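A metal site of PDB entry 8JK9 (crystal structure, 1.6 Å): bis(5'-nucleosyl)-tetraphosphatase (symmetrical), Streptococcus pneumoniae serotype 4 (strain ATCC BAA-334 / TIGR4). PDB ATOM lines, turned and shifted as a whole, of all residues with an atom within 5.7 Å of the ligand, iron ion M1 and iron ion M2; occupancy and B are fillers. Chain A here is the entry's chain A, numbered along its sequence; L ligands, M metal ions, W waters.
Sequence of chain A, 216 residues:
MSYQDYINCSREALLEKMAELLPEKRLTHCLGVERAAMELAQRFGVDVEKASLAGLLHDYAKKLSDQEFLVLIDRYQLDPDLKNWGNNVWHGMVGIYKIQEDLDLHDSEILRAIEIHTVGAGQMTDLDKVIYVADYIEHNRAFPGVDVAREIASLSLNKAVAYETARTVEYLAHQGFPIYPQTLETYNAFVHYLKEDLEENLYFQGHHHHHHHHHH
Thr 118 touches iron ion M2.
Arg 141 touches iron ion M1.
Five residues have an atom within 4 Å of iron ion M1: His 29, His 58, Asp 59, Asp 135 and Arg 141.
O of Glu 164 is in hydrogen-bond range of OG1 of Thr 168.
The backbone NH (N) of Phe 177 lies within hydrogen-bond range of the backbone carbonyl oxygen (O) of Leu 172 (2.9 Å).
The side-chain carboxylate (OD2) of Asp 59 sits close to the guanidinium group (NH2) of Arg 26, 3.1 Å away.
The guanidinium group of Arg 141 lies within salt-bridge range of the side-chain carboxylate of Asp 135 (3.9 Å).
A ring nitrogen (ND1) of His 91 lies within hydrogen-bond range of the backbone carbonyl oxygen of Asn 88, 3.2 Å away.
The side-chain hydroxyl (OG1) of Thr 118 lies close to a ring nitrogen (NE2) of His 117.
Iron ion M1 is bound by water W2 (2.0 Å), a ring nitrogen (NE2) of His 29 (2.1 Å), an oxygen (O1) of the ligand (2.1 Å), the side-chain carboxylate of Asp 59 (2.2 Å), a ring nitrogen (NE2) of His 58 (2.2 Å) and the side-chain carboxylate of Asp 135 (2.2 Å).
Thr 168 touches the ligand (CG2 to C6, 3.9 Å).
CD1 of Leu 172 touches C8 of the ligand (3.5 Å).
CA of Ile 179 touches O11 of the ligand (3.7 Å).
Iron ion M2 is bound by water W2 (1.9 Å), the side-chain carboxylate (OD1) of Asp 59 (2.1 Å), a ring nitrogen (NE2) of His 91 (2.1 Å), an oxygen (O3) of the ligand (2.1 Å), an oxygen (O5) of the ligand (2.2 Å) and a ring nitrogen (NE2) of His 117 (2.2 Å).
Iron ion M2 has six donor atoms within binding distance.
O of Pro 178 sits at hydrogen-bond distance from N3 of the ligand, at 2.9 Å.
The side-chain amide nitrogen of Asn 88 is in hydrogen-bond range of a nitrogen (N5) of the ligand (3.3 Å).
The side-chain hydroxyl (OG1) of Thr 183 is in hydrogen-bond range of an oxygen (O11) of the ligand (2.9 Å).
NH2 of Arg 26 is in salt-bridge range of O2 of the ligand, 3.5 Å away.
An oxygen (O11) of the ligand sits at hydrogen-bond distance from the backbone NH (N) of Tyr 180.
The side-chain hydroxyl (OG1) of Thr 118 sits close to an oxygen (O5) of the ligand, 2.7 Å away.
The guanidinium group of Arg 141 lies within salt-bridge range of an oxygen (O2) of the ligand (3.998 Å).
An oxygen (O2) of the ligand is in salt-bridge range of the side-chain amino group (NZ) of Lys 62.
Water W2 bridges the side-chain carboxylate of Asp 135 (2.7 Å) and an oxygen (O4) of the ligand (3.0 Å).
Water W7 lies within hydrogen-bond range of O2 of the ligand (2.6 Å), NH2 of Arg 141 (3.0 Å) and NH1 of Arg 26 (3.0 Å).
Water W1 bridges an oxygen (O6) of the ligand (2.6 Å) and the backbone carbonyl oxygen (O) of Thr 118 (2.9 Å).
Water W5 lies within hydrogen-bond range of the backbone carbonyl oxygen (O) of Thr 118 and a nitrogen (N2) of the ligand.
Water W8 lies within hydrogen-bond range of the guanidinium group of Arg 141 (3.0 Å), the side-chain carboxylate of Asp 135 (3.0 Å) and an oxygen (O6) of the ligand (3.2 Å).
Water W9 lies within hydrogen-bond range of NZ of Lys 62 and O2 of the ligand.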
ATOM      1  N   ARG A  26      -5.876  20.071 -13.237  1.00  0.00           N
ATOM      2  CA  ARG A  26      -7.043  20.943 -13.152  1.00  0.00           C
ATOM      3  C   ARG A  26      -6.649  22.425 -13.200  1.00  0.00           C
ATOM      4  O   ARG A  26      -7.332  23.202 -13.864  1.00  0.00           O
ATOM      5  CB  ARG A  26      -7.883  20.634 -11.897  1.00  0.00           C
ATOM      6  CG  ARG A  26      -9.213  21.393 -11.767  1.00  0.00           C
ATOM      7  CD  ARG A  26     -10.153  21.192 -12.946  1.00  0.00           C
ATOM      8  NE  ARG A  26     -10.360  19.768 -13.236  1.00  0.00           N
ATOM      9  CZ  ARG A  26     -11.119  19.297 -14.225  1.00  0.00           C
ATOM     10  NH1 ARG A  26     -11.230  17.986 -14.388  1.00  0.00           N
ATOM     11  NH2 ARG A  26     -11.763  20.117 -15.044  1.00  0.00           N
ATOM     12  N   HIS A  29      -5.743  23.201 -16.733  1.00  0.00           N
ATOM     13  CA  HIS A  29      -7.000  23.380 -17.452  1.00  0.00           C
ATOM     14  C   HIS A  29      -7.562  24.788 -17.236  1.00  0.00           C
ATOM     15  O   HIS A  29      -7.900  25.456 -18.206  1.00  0.00           O
ATOM     16  CB  HIS A  29      -7.997  22.267 -17.047  1.00  0.00           C
ATOM     17  CG  HIS A  29      -9.425  22.568 -17.399  1.00  0.00           C
ATOM     18  ND1 HIS A  29      -9.876  22.578 -18.700  1.00  0.00           N
ATOM     19  CD2 HIS A  29     -10.503  22.842 -16.621  1.00  0.00           C
ATOM     20  CE1 HIS A  29     -11.168  22.866 -18.710  1.00  0.00           C
ATOM     21  NE2 HIS A  29     -11.571  23.021 -17.464  1.00  0.00           N
ATOM     22  N   VAL A  33      -8.406  27.641 -20.000  1.00  0.00           N
ATOM     23  CA  VAL A  33      -9.703  28.310 -20.158  1.00  0.00           C
ATOM     24  C   VAL A  33      -9.554  29.839 -20.065  1.00  0.00           C
ATOM     25  O   VAL A  33     -10.187  30.566 -20.820  1.00  0.00           O
ATOM     26  CB  VAL A  33     -10.748  27.740 -19.157  1.00  0.00           C
ATOM     27  CG1 VAL A  33     -12.107  28.424 -19.311  1.00  0.00           C
ATOM     28  CG2 VAL A  33     -10.916  26.255 -19.383  1.00  0.00           C
ATOM     29  N   HIS A  58     -13.440  29.267 -13.298  1.00  0.00           N
ATOM     30  CA  HIS A  58     -14.681  28.515 -13.540  1.00  0.00           C
ATOM     31  C   HIS A  58     -14.720  27.168 -12.790  1.00  0.00           C
ATOM     32  O   HIS A  58     -15.783  26.780 -12.282  1.00  0.00           O
ATOM     33  CB  HIS A  58     -14.941  28.321 -15.038  1.00  0.00           C
ATOM     34  CG  HIS A  58     -14.159  27.200 -15.628  1.00  0.00           C
ATOM     35  ND1 HIS A  58     -12.808  27.277 -15.875  1.00  0.00           N
ATOM     36  CD2 HIS A  58     -14.538  25.945 -15.969  1.00  0.00           C
ATOM     37  CE1 HIS A  58     -12.386  26.122 -16.361  1.00  0.00           C
ATOM     38  NE2 HIS A  58     -13.419  25.306 -16.432  1.00  0.00           N
ATOM     39  N   ASP A  59     -13.566  26.498 -12.668  1.00  0.00           N
ATOM     40  CA  ASP A  59     -13.470  25.216 -11.968  1.00  0.00           C
ATOM     41  C   ASP A  59     -12.826  25.302 -10.574  1.00  0.00           C
ATOM     42  O   ASP A  59     -12.361  24.283 -10.038  1.00  0.00           O
ATOM     43  CB  ASP A  59     -12.731  24.158 -12.826  1.00  0.00           C
ATOM     44  CG  ASP A  59     -13.645  23.448 -13.820  1.00  0.00           C
ATOM     45  OD1 ASP A  59     -14.891  23.477 -13.677  1.00  0.00           O
ATOM     46  OD2 ASP A  59     -13.090  22.864 -14.777  1.00  0.00           O
ATOM     47  N   LYS A  62     -14.107  22.702  -8.144  1.00  0.00           N
ATOM     48  CA  LYS A  62     -14.185  21.337  -8.681  1.00  0.00           C
ATOM     49  C   LYS A  62     -13.972  20.232  -7.640  1.00  0.00           C
ATOM     50  O   LYS A  62     -14.549  19.140  -7.755  1.00  0.00           O
ATOM     51  CB  LYS A  62     -13.191  21.170  -9.832  1.00  0.00           C
ATOM     52  CG  LYS A  62     -13.257  19.852 -10.577  1.00  0.00           C
ATOM     53  CD  LYS A  62     -14.406  19.795 -11.575  1.00  0.00           C
ATOM     54  CE  LYS A  62     -14.275  18.607 -12.504  1.00  0.00           C
ATOM     55  NZ  LYS A  62     -15.432  18.548 -13.456  1.00  0.00           N
ATOM     56  N   TRP A  85     -28.430  15.695  -7.102  1.00  0.00           N
ATOM     57  CA  TRP A  85     -27.422  15.663  -8.167  1.00  0.00           C
ATOM     58  C   TRP A  85     -26.029  15.473  -7.550  1.00  0.00           C
ATOM     59  O   TRP A  85     -25.901  14.804  -6.514  1.00  0.00           O
ATOM     60  CB  TRP A  85     -27.579  16.896  -9.087  1.00  0.00           C
ATOM     61  CG  TRP A  85     -28.950  16.912  -9.731  1.00  0.00           C
ATOM     62  CD1 TRP A  85     -30.085  17.463  -9.204  1.00  0.00           C
ATOM     63  CD2 TRP A  85     -29.336  16.290 -10.955  1.00  0.00           C
ATOM     64  NE1 TRP A  85     -31.153  17.257 -10.043  1.00  0.00           N
ATOM     65  CE2 TRP A  85     -30.727  16.532 -11.122  1.00  0.00           C
ATOM     66  CE3 TRP A  85     -28.645  15.575 -11.937  1.00  0.00           C
ATOM     67  CZ2 TRP A  85     -31.432  16.073 -12.237  1.00  0.00           C
ATOM     68  CZ3 TRP A  85     -29.362  15.126 -13.058  1.00  0.00           C
ATOM     69  CH2 TRP A  85     -30.732  15.369 -13.184  1.00  0.00           C
ATOM     70  N   ASN A  88     -20.846  17.318 -10.805  1.00  0.00           N
ATOM     71  CA  ASN A  88     -21.026  17.865 -12.158  1.00  0.00           C
ATOM     72  C   ASN A  88     -21.921  19.101 -12.193  1.00  0.00           C
ATOM     73  O   ASN A  88     -21.545  20.131 -12.746  1.00  0.00           O
ATOM     74  CB  ASN A  88     -21.541  16.799 -13.131  1.00  0.00           C
ATOM     75  CG  ASN A  88     -20.487  15.745 -13.459  1.00  0.00           C
ATOM     76  OD1 ASN A  88     -19.328  15.850 -13.061  1.00  0.00           O
ATOM     77  ND2 ASN A  88     -20.899  14.721 -14.212  1.00  0.00           N
ATOM     78  N   VAL A  89     -23.090  18.992 -11.551  1.00  0.00           N
ATOM     79  CA  VAL A  89     -24.013  20.121 -11.431  1.00  0.00           C
ATOM     80  C   VAL A  89     -23.502  21.127 -10.387  1.00  0.00           C
ATOM     81  O   VAL A  89     -23.525  22.330 -10.629  1.00  0.00           O
ATOM     82  CB  VAL A  89     -25.450  19.629 -11.089  1.00  0.00           C
ATOM     83  CG1 VAL A  89     -26.381  20.811 -10.831  1.00  0.00           C
ATOM     84  CG2 VAL A  89     -26.004  18.788 -12.227  1.00  0.00           C
ATOM     85  N   HIS A  91     -20.470  22.019  -8.994  1.00  0.00           N
ATOM     86  CA  HIS A  91     -19.204  22.771  -8.901  1.00  0.00           C
ATOM     87  C   HIS A  91     -19.322  24.182  -9.464  1.00  0.00           C
ATOM     88  O   HIS A  91     -18.687  25.105  -8.949  1.00  0.00           O
ATOM     89  CB  HIS A  91     -17.970  22.000  -9.395  1.00  0.00           C
ATOM     90  CG  HIS A  91     -17.861  21.869 -10.888  1.00  0.00           C
ATOM     91  ND1 HIS A  91     -18.645  21.015 -11.620  1.00  0.00           N
ATOM     92  CD2 HIS A  91     -17.033  22.481 -11.765  1.00  0.00           C
ATOM     93  CE1 HIS A  91     -18.322  21.110 -12.903  1.00  0.00           C
ATOM     94  NE2 HIS A  91     -17.347  21.992 -13.013  1.00  0.00           N
ATOM     95  N   HIS A 117     -21.566  27.361 -16.247  1.00  0.00           N
ATOM     96  CA  HIS A 117     -20.525  26.935 -17.209  1.00  0.00           C
ATOM     97  C   HIS A 117     -20.644  25.466 -17.660  1.00  0.00           C
ATOM     98  O   HIS A 117     -20.156  25.111 -18.729  1.00  0.00           O
ATOM     99  CB  HIS A 117     -19.108  27.221 -16.706  1.00  0.00           C
ATOM    100  CG  HIS A 117     -18.549  26.159 -15.811  1.00  0.00           C
ATOM    101  ND1 HIS A 117     -18.638  26.229 -14.432  1.00  0.00           N
ATOM    102  CD2 HIS A 117     -17.893  25.004 -16.085  1.00  0.00           C
ATOM    103  CE1 HIS A 117     -18.066  25.167 -13.895  1.00  0.00           C
ATOM    104  NE2 HIS A 117     -17.604  24.412 -14.886  1.00  0.00           N
ATOM    105  N   THR A 118     -21.242  24.637 -16.818  1.00  0.00           N
ATOM    106  CA  THR A 118     -21.364  23.206 -17.130  1.00  0.00           C
ATOM    107  C   THR A 118     -22.640  22.915 -17.932  1.00  0.00           C
ATOM    108  O   THR A 118     -22.597  22.222 -18.959  1.00  0.00           O
ATOM    109  CB  THR A 118     -21.387  22.340 -15.853  1.00  0.00           C
ATOM    110  OG1 THR A 118     -20.251  22.647 -15.030  1.00  0.00           O
ATOM    111  CG2 THR A 118     -21.432  20.855 -16.169  1.00  0.00           C
ATOM    112  N   VAL A 119     -23.762  23.455 -17.451  1.00  0.00           N
ATOM    113  CA  VAL A 119     -25.080  23.116 -17.969  1.00  0.00           C
ATOM    114  C   VAL A 119     -25.666  24.144 -18.952  1.00  0.00           C
ATOM    115  O   VAL A 119     -26.583  23.822 -19.707  1.00  0.00           O
ATOM    116  CB  VAL A 119     -26.080  22.828 -16.809  1.00  0.00           C
ATOM    117  CG1 VAL A 119     -25.589  21.649 -15.989  1.00  0.00           C
ATOM    118  CG2 VAL A 119     -26.289  24.053 -15.917  1.00  0.00           C
ATOM    119  N   ASP A 135     -14.229  26.553 -22.045  1.00  0.00           N
ATOM    120  CA  ASP A 135     -14.040  25.367 -21.240  1.00  0.00           C
ATOM    121  C   ASP A 135     -13.845  24.107 -22.098  1.00  0.00           C
ATOM    122  O   ASP A 135     -13.019  23.249 -21.801  1.00  0.00           O
ATOM    123  CB  ASP A 135     -15.256  25.222 -20.333  1.00  0.00           C
ATOM    124  CG  ASP A 135     -15.133  24.090 -19.351  1.00  0.00           C
ATOM    125  OD1 ASP A 135     -14.010  23.775 -18.904  1.00  0.00           O
ATOM    126  OD2 ASP A 135     -16.187  23.529 -19.009  1.00  0.00           O
ATOM    127  N   ARG A 141      -7.371  20.303 -23.914  1.00  0.00           N
ATOM    128  CA  ARG A 141      -8.414  19.322 -24.215  1.00  0.00           C
ATOM    129  C   ARG A 141      -8.047  18.490 -25.421  1.00  0.00           C
ATOM    130  O   ARG A 141      -7.576  19.013 -26.441  1.00  0.00           O
ATOM    131  CB  ARG A 141      -9.784  19.978 -24.443  1.00  0.00           C
ATOM    132  CG  ARG A 141     -10.401  20.686 -23.246  1.00  0.00           C
ATOM    133  CD  ARG A 141     -11.096  19.717 -22.295  1.00  0.00           C
ATOM    134  NE  ARG A 141     -12.172  20.384 -21.560  1.00  0.00           N
ATOM    135  CZ  ARG A 141     -12.480  20.167 -20.287  1.00  0.00           C
ATOM    136  NH1 ARG A 141     -13.487  20.841 -19.730  1.00  0.00           N
ATOM    137  NH2 ARG A 141     -11.801  19.291 -19.553  1.00  0.00           N
ATOM    138  N   GLU A 164     -21.494  22.047 -28.694  1.00  0.00           N
ATOM    139  CA  GLU A 164     -21.098  21.496 -27.395  1.00  0.00           C
ATOM    140  C   GLU A 164     -22.285  20.869 -26.645  1.00  0.00           C
ATOM    141  O   GLU A 164     -22.175  19.740 -26.125  1.00  0.00           O
ATOM    142  CB  GLU A 164     -20.410  22.557 -26.540  1.00  0.00           C
ATOM    143  CG  GLU A 164     -20.102  22.051 -25.134  1.00  0.00           C
ATOM    144  CD  GLU A 164     -19.408  23.061 -24.243  1.00  0.00           C
ATOM    145  OE1 GLU A 164     -19.057  24.158 -24.727  1.00  0.00           O
ATOM    146  OE2 GLU A 164     -19.225  22.732 -23.054  1.00  0.00           O
ATOM    147  N   THR A 168     -22.756  16.972 -25.727  1.00  0.00           N
ATOM    148  CA  THR A 168     -22.861  16.613 -24.305  1.00  0.00           C
ATOM    149  C   THR A 168     -24.111  15.783 -24.004  1.00  0.00           C
ATOM    150  O   THR A 168     -24.011  14.735 -23.358  1.00  0.00           O
ATOM    151  CB  THR A 168     -22.758  17.864 -23.437  1.00  0.00           C
ATOM    152  OG1 THR A 168     -21.444  18.403 -23.642  1.00  0.00           O
ATOM    153  CG2 THR A 168     -22.913  17.511 -21.952  1.00  0.00           C
ATOM    154  N   LEU A 172     -24.045  11.955 -22.739  1.00  0.00           N
ATOM    155  CA  LEU A 172     -24.682  11.578 -21.474  1.00  0.00           C
ATOM    156  C   LEU A 172     -25.643  10.409 -21.686  1.00  0.00           C
ATOM    157  O   LEU A 172     -25.626   9.439 -20.903  1.00  0.00           O
ATOM    158  CB  LEU A 172     -25.386  12.781 -20.837  1.00  0.00           C
ATOM    159  CG  LEU A 172     -24.465  13.871 -20.297  1.00  0.00           C
ATOM    160  CD1 LEU A 172     -25.298  15.119 -20.060  1.00  0.00           C
ATOM    161  CD2 LEU A 172     -23.721  13.427 -19.040  1.00  0.00           C
ATOM    162  N   PHE A 177     -26.120   8.380 -18.204  1.00  0.00           N
ATOM    163  CA  PHE A 177     -26.102   9.279 -17.052  1.00  0.00           C
ATOM    164  C   PHE A 177     -27.299  10.222 -17.049  1.00  0.00           C
ATOM    165  O   PHE A 177     -27.741  10.646 -18.122  1.00  0.00           O
ATOM    166  CB  PHE A 177     -24.825  10.132 -17.058  1.00  0.00           C
ATOM    167  CG  PHE A 177     -23.533   9.338 -17.003  1.00  0.00           C
ATOM    168  CD1 PHE A 177     -23.464   8.106 -16.344  1.00  0.00           C
ATOM    169  CD2 PHE A 177     -22.382   9.857 -17.585  1.00  0.00           C
ATOM    170  CE1 PHE A 177     -22.257   7.401 -16.291  1.00  0.00           C
ATOM    171  CE2 PHE A 177     -21.173   9.160 -17.521  1.00  0.00           C
ATOM    172  CZ  PHE A 177     -21.117   7.938 -16.885  1.00  0.00           C
ATOM    173  N   PRO A 178     -27.826  10.571 -15.859  1.00  0.00           N
ATOM    174  CA  PRO A 178     -28.958  11.517 -15.786  1.00  0.00           C
ATOM    175  C   PRO A 178     -28.611  12.882 -16.382  1.00  0.00           C
ATOM    176  O   PRO A 178     -27.489  13.340 -16.213  1.00  0.00           O
ATOM    177  CB  PRO A 178     -29.231  11.663 -14.278  1.00  0.00           C
ATOM    178  CG  PRO A 178     -28.446  10.600 -13.604  1.00  0.00           C
ATOM    179  CD  PRO A 178     -27.398  10.086 -14.531  1.00  0.00           C
ATOM    180  N   ILE A 179     -29.578  13.501 -17.060  1.00  0.00           N
ATOM    181  CA  ILE A 179     -29.359  14.780 -17.738  1.00  0.00           C
ATOM    182  C   ILE A 179     -30.090  15.840 -16.927  1.00  0.00           C
ATOM    183  O   ILE A 179     -31.302  15.769 -16.759  1.00  0.00           O
ATOM    184  CB  ILE A 179     -29.860  14.731 -19.200  1.00  0.00           C
ATOM    185  CG1 ILE A 179     -29.009  13.746 -19.999  1.00  0.00           C
ATOM    186  CG2 ILE A 179     -29.852  16.121 -19.848  1.00  0.00           C
ATOM    187  CD1 ILE A 179     -29.635  13.268 -21.291  1.00  0.00           C
ATOM    188  N   TYR A 180     -29.330  16.817 -16.445  1.00  0.00           N
ATOM    189  CA  TYR A 180     -29.904  17.912 -15.667  1.00  0.00           C
ATOM    190  C   TYR A 180     -30.927  18.697 -16.491  1.00  0.00           C
ATOM    191  O   TYR A 180     -30.660  19.021 -17.645  1.00  0.00           O
ATOM    192  CB  TYR A 180     -28.781  18.836 -15.150  1.00  0.00           C
ATOM    193  CG  TYR A 180     -29.232  19.792 -14.086  1.00  0.00           C
ATOM    194  CD1 TYR A 180     -29.756  19.313 -12.882  1.00  0.00           C
ATOM    195  CD2 TYR A 180     -29.098  21.168 -14.258  1.00  0.00           C
ATOM    196  CE1 TYR A 180     -30.167  20.201 -11.886  1.00  0.00           C
ATOM    197  CE2 TYR A 180     -29.508  22.064 -13.267  1.00  0.00           C
ATOM    198  CZ  TYR A 180     -30.033  21.576 -12.092  1.00  0.00           C
ATOM    199  OH  TYR A 180     -30.426  22.485 -11.131  1.00  0.00           O
ATOM    200  N   THR A 183     -29.687  21.604 -18.543  1.00  0.00           N
ATOM    201  CA  THR A 183     -28.946  21.160 -19.741  1.00  0.00           C
ATOM    202  C   THR A 183     -29.872  21.040 -20.960  1.00  0.00           C
ATOM    203  O   THR A 183     -29.529  21.476 -22.062  1.00  0.00           O
ATOM    204  CB  THR A 183     -28.206  19.833 -19.458  1.00  0.00           C
ATOM    205  OG1 THR A 183     -27.253  20.059 -18.413  1.00  0.00           O
ATOM    206  CG2 THR A 183     -27.471  19.311 -20.696  1.00  0.00           C
HETATM  207  P1  LIG L   1     -14.948  20.277 -16.455  1.00  0.00           P
HETATM  208  O1  LIG L   1     -13.827  21.077 -17.087  1.00  0.00           O
HETATM  209  O2  LIG L   1     -14.675  18.785 -16.513  1.00  0.00           O
HETATM  210  O3  LIG L   1     -15.368  20.767 -15.080  1.00  0.00           O
HETATM  211  O4  LIG L   1     -16.179  20.445 -17.491  1.00  0.00           O
HETATM  212  P2  LIG L   1     -17.739  20.751 -17.199  1.00  0.00           P
HETATM  213  O5  LIG L   1     -17.925  21.553 -15.939  1.00  0.00           O
HETATM  214  O6  LIG L   1     -18.370  21.268 -18.466  1.00  0.00           O
HETATM  215  O7  LIG L   1     -18.383  19.292 -16.994  1.00  0.00           O
HETATM  216  C1  LIG L   1     -18.018  18.363 -15.998  1.00  0.00           C
HETATM  217  C2  LIG L   1     -18.765  17.055 -16.263  1.00  0.00           C
HETATM  218  O8  LIG L   1     -20.161  17.337 -16.101  1.00  0.00           O
HETATM  219  C3  LIG L   1     -18.576  16.464 -17.664  1.00  0.00           C
HETATM  220  O9  LIG L   1     -18.263  15.058 -17.560  1.00  0.00           O
HETATM  221  C4  LIG L   1     -19.918  16.694 -18.332  1.00  0.00           C
HETATM  222  O10 LIG L   1     -20.261  15.752 -19.351  1.00  0.00           O
HETATM  223  C5  LIG L   1     -20.845  16.631 -17.121  1.00  0.00           C
HETATM  224  N1  LIG L   1     -22.214  17.121 -17.371  1.00  0.00           N
HETATM  225  C6  LIG L   1     -22.580  18.196 -18.096  1.00  0.00           C
HETATM  226  N2  LIG L   1     -23.930  18.312 -18.117  1.00  0.00           N
HETATM  227  C7  LIG L   1     -24.411  17.276 -17.410  1.00  0.00           C
HETATM  228  C8  LIG L   1     -25.734  16.781 -17.027  1.00  0.00           C
HETATM  229  O11 LIG L   1     -26.747  17.372 -17.411  1.00  0.00           O
HETATM  230  N3  LIG L   1     -25.792  15.653 -16.290  1.00  0.00           N
HETATM  231  C9  LIG L   1     -24.693  14.982 -15.875  1.00  0.00           C
HETATM  232  N4  LIG L   1     -24.837  13.860 -15.134  1.00  0.00           N
HETATM  233  N5  LIG L   1     -23.436  15.393 -16.167  1.00  0.00           N
HETATM  234  C10 LIG L   1     -23.272  16.507 -16.913  1.00  0.00           C
HETATM  235 FE    FE M   1     -13.589  23.191 -16.854  1.00  0.00          FE
HETATM  236 FE    FE M   2     -16.419  22.598 -14.800  1.00  0.00          FE
HETATM  237 MG    MG M   3     -21.457  23.003 -12.609  1.00  0.00          MG
HETATM  238  O   HOH W   1     -20.499  20.344 -19.713  1.00  0.00           O
HETATM  239  O   HOH W   2     -15.540  23.151 -16.415  1.00  0.00           O
HETATM  240  O   HOH W   3     -20.735  12.806 -17.247  1.00  0.00           O
HETATM  241  O   HOH W   4     -18.621  23.509 -20.361  1.00  0.00           O
HETATM  242  O   HOH W   5     -24.175  20.274 -20.206  1.00  0.00           O
HETATM  243  O   HOH W   6     -15.168  17.477 -19.188  1.00  0.00           O
HETATM  244  O   HOH W   7     -12.378  17.677 -17.122  1.00  0.00           O
HETATM  245  O   HOH W   8     -16.235  21.153 -20.842  1.00  0.00           O
HETATM  246  O   HOH W   9     -15.066  15.847 -14.979  1.00  0.00           O
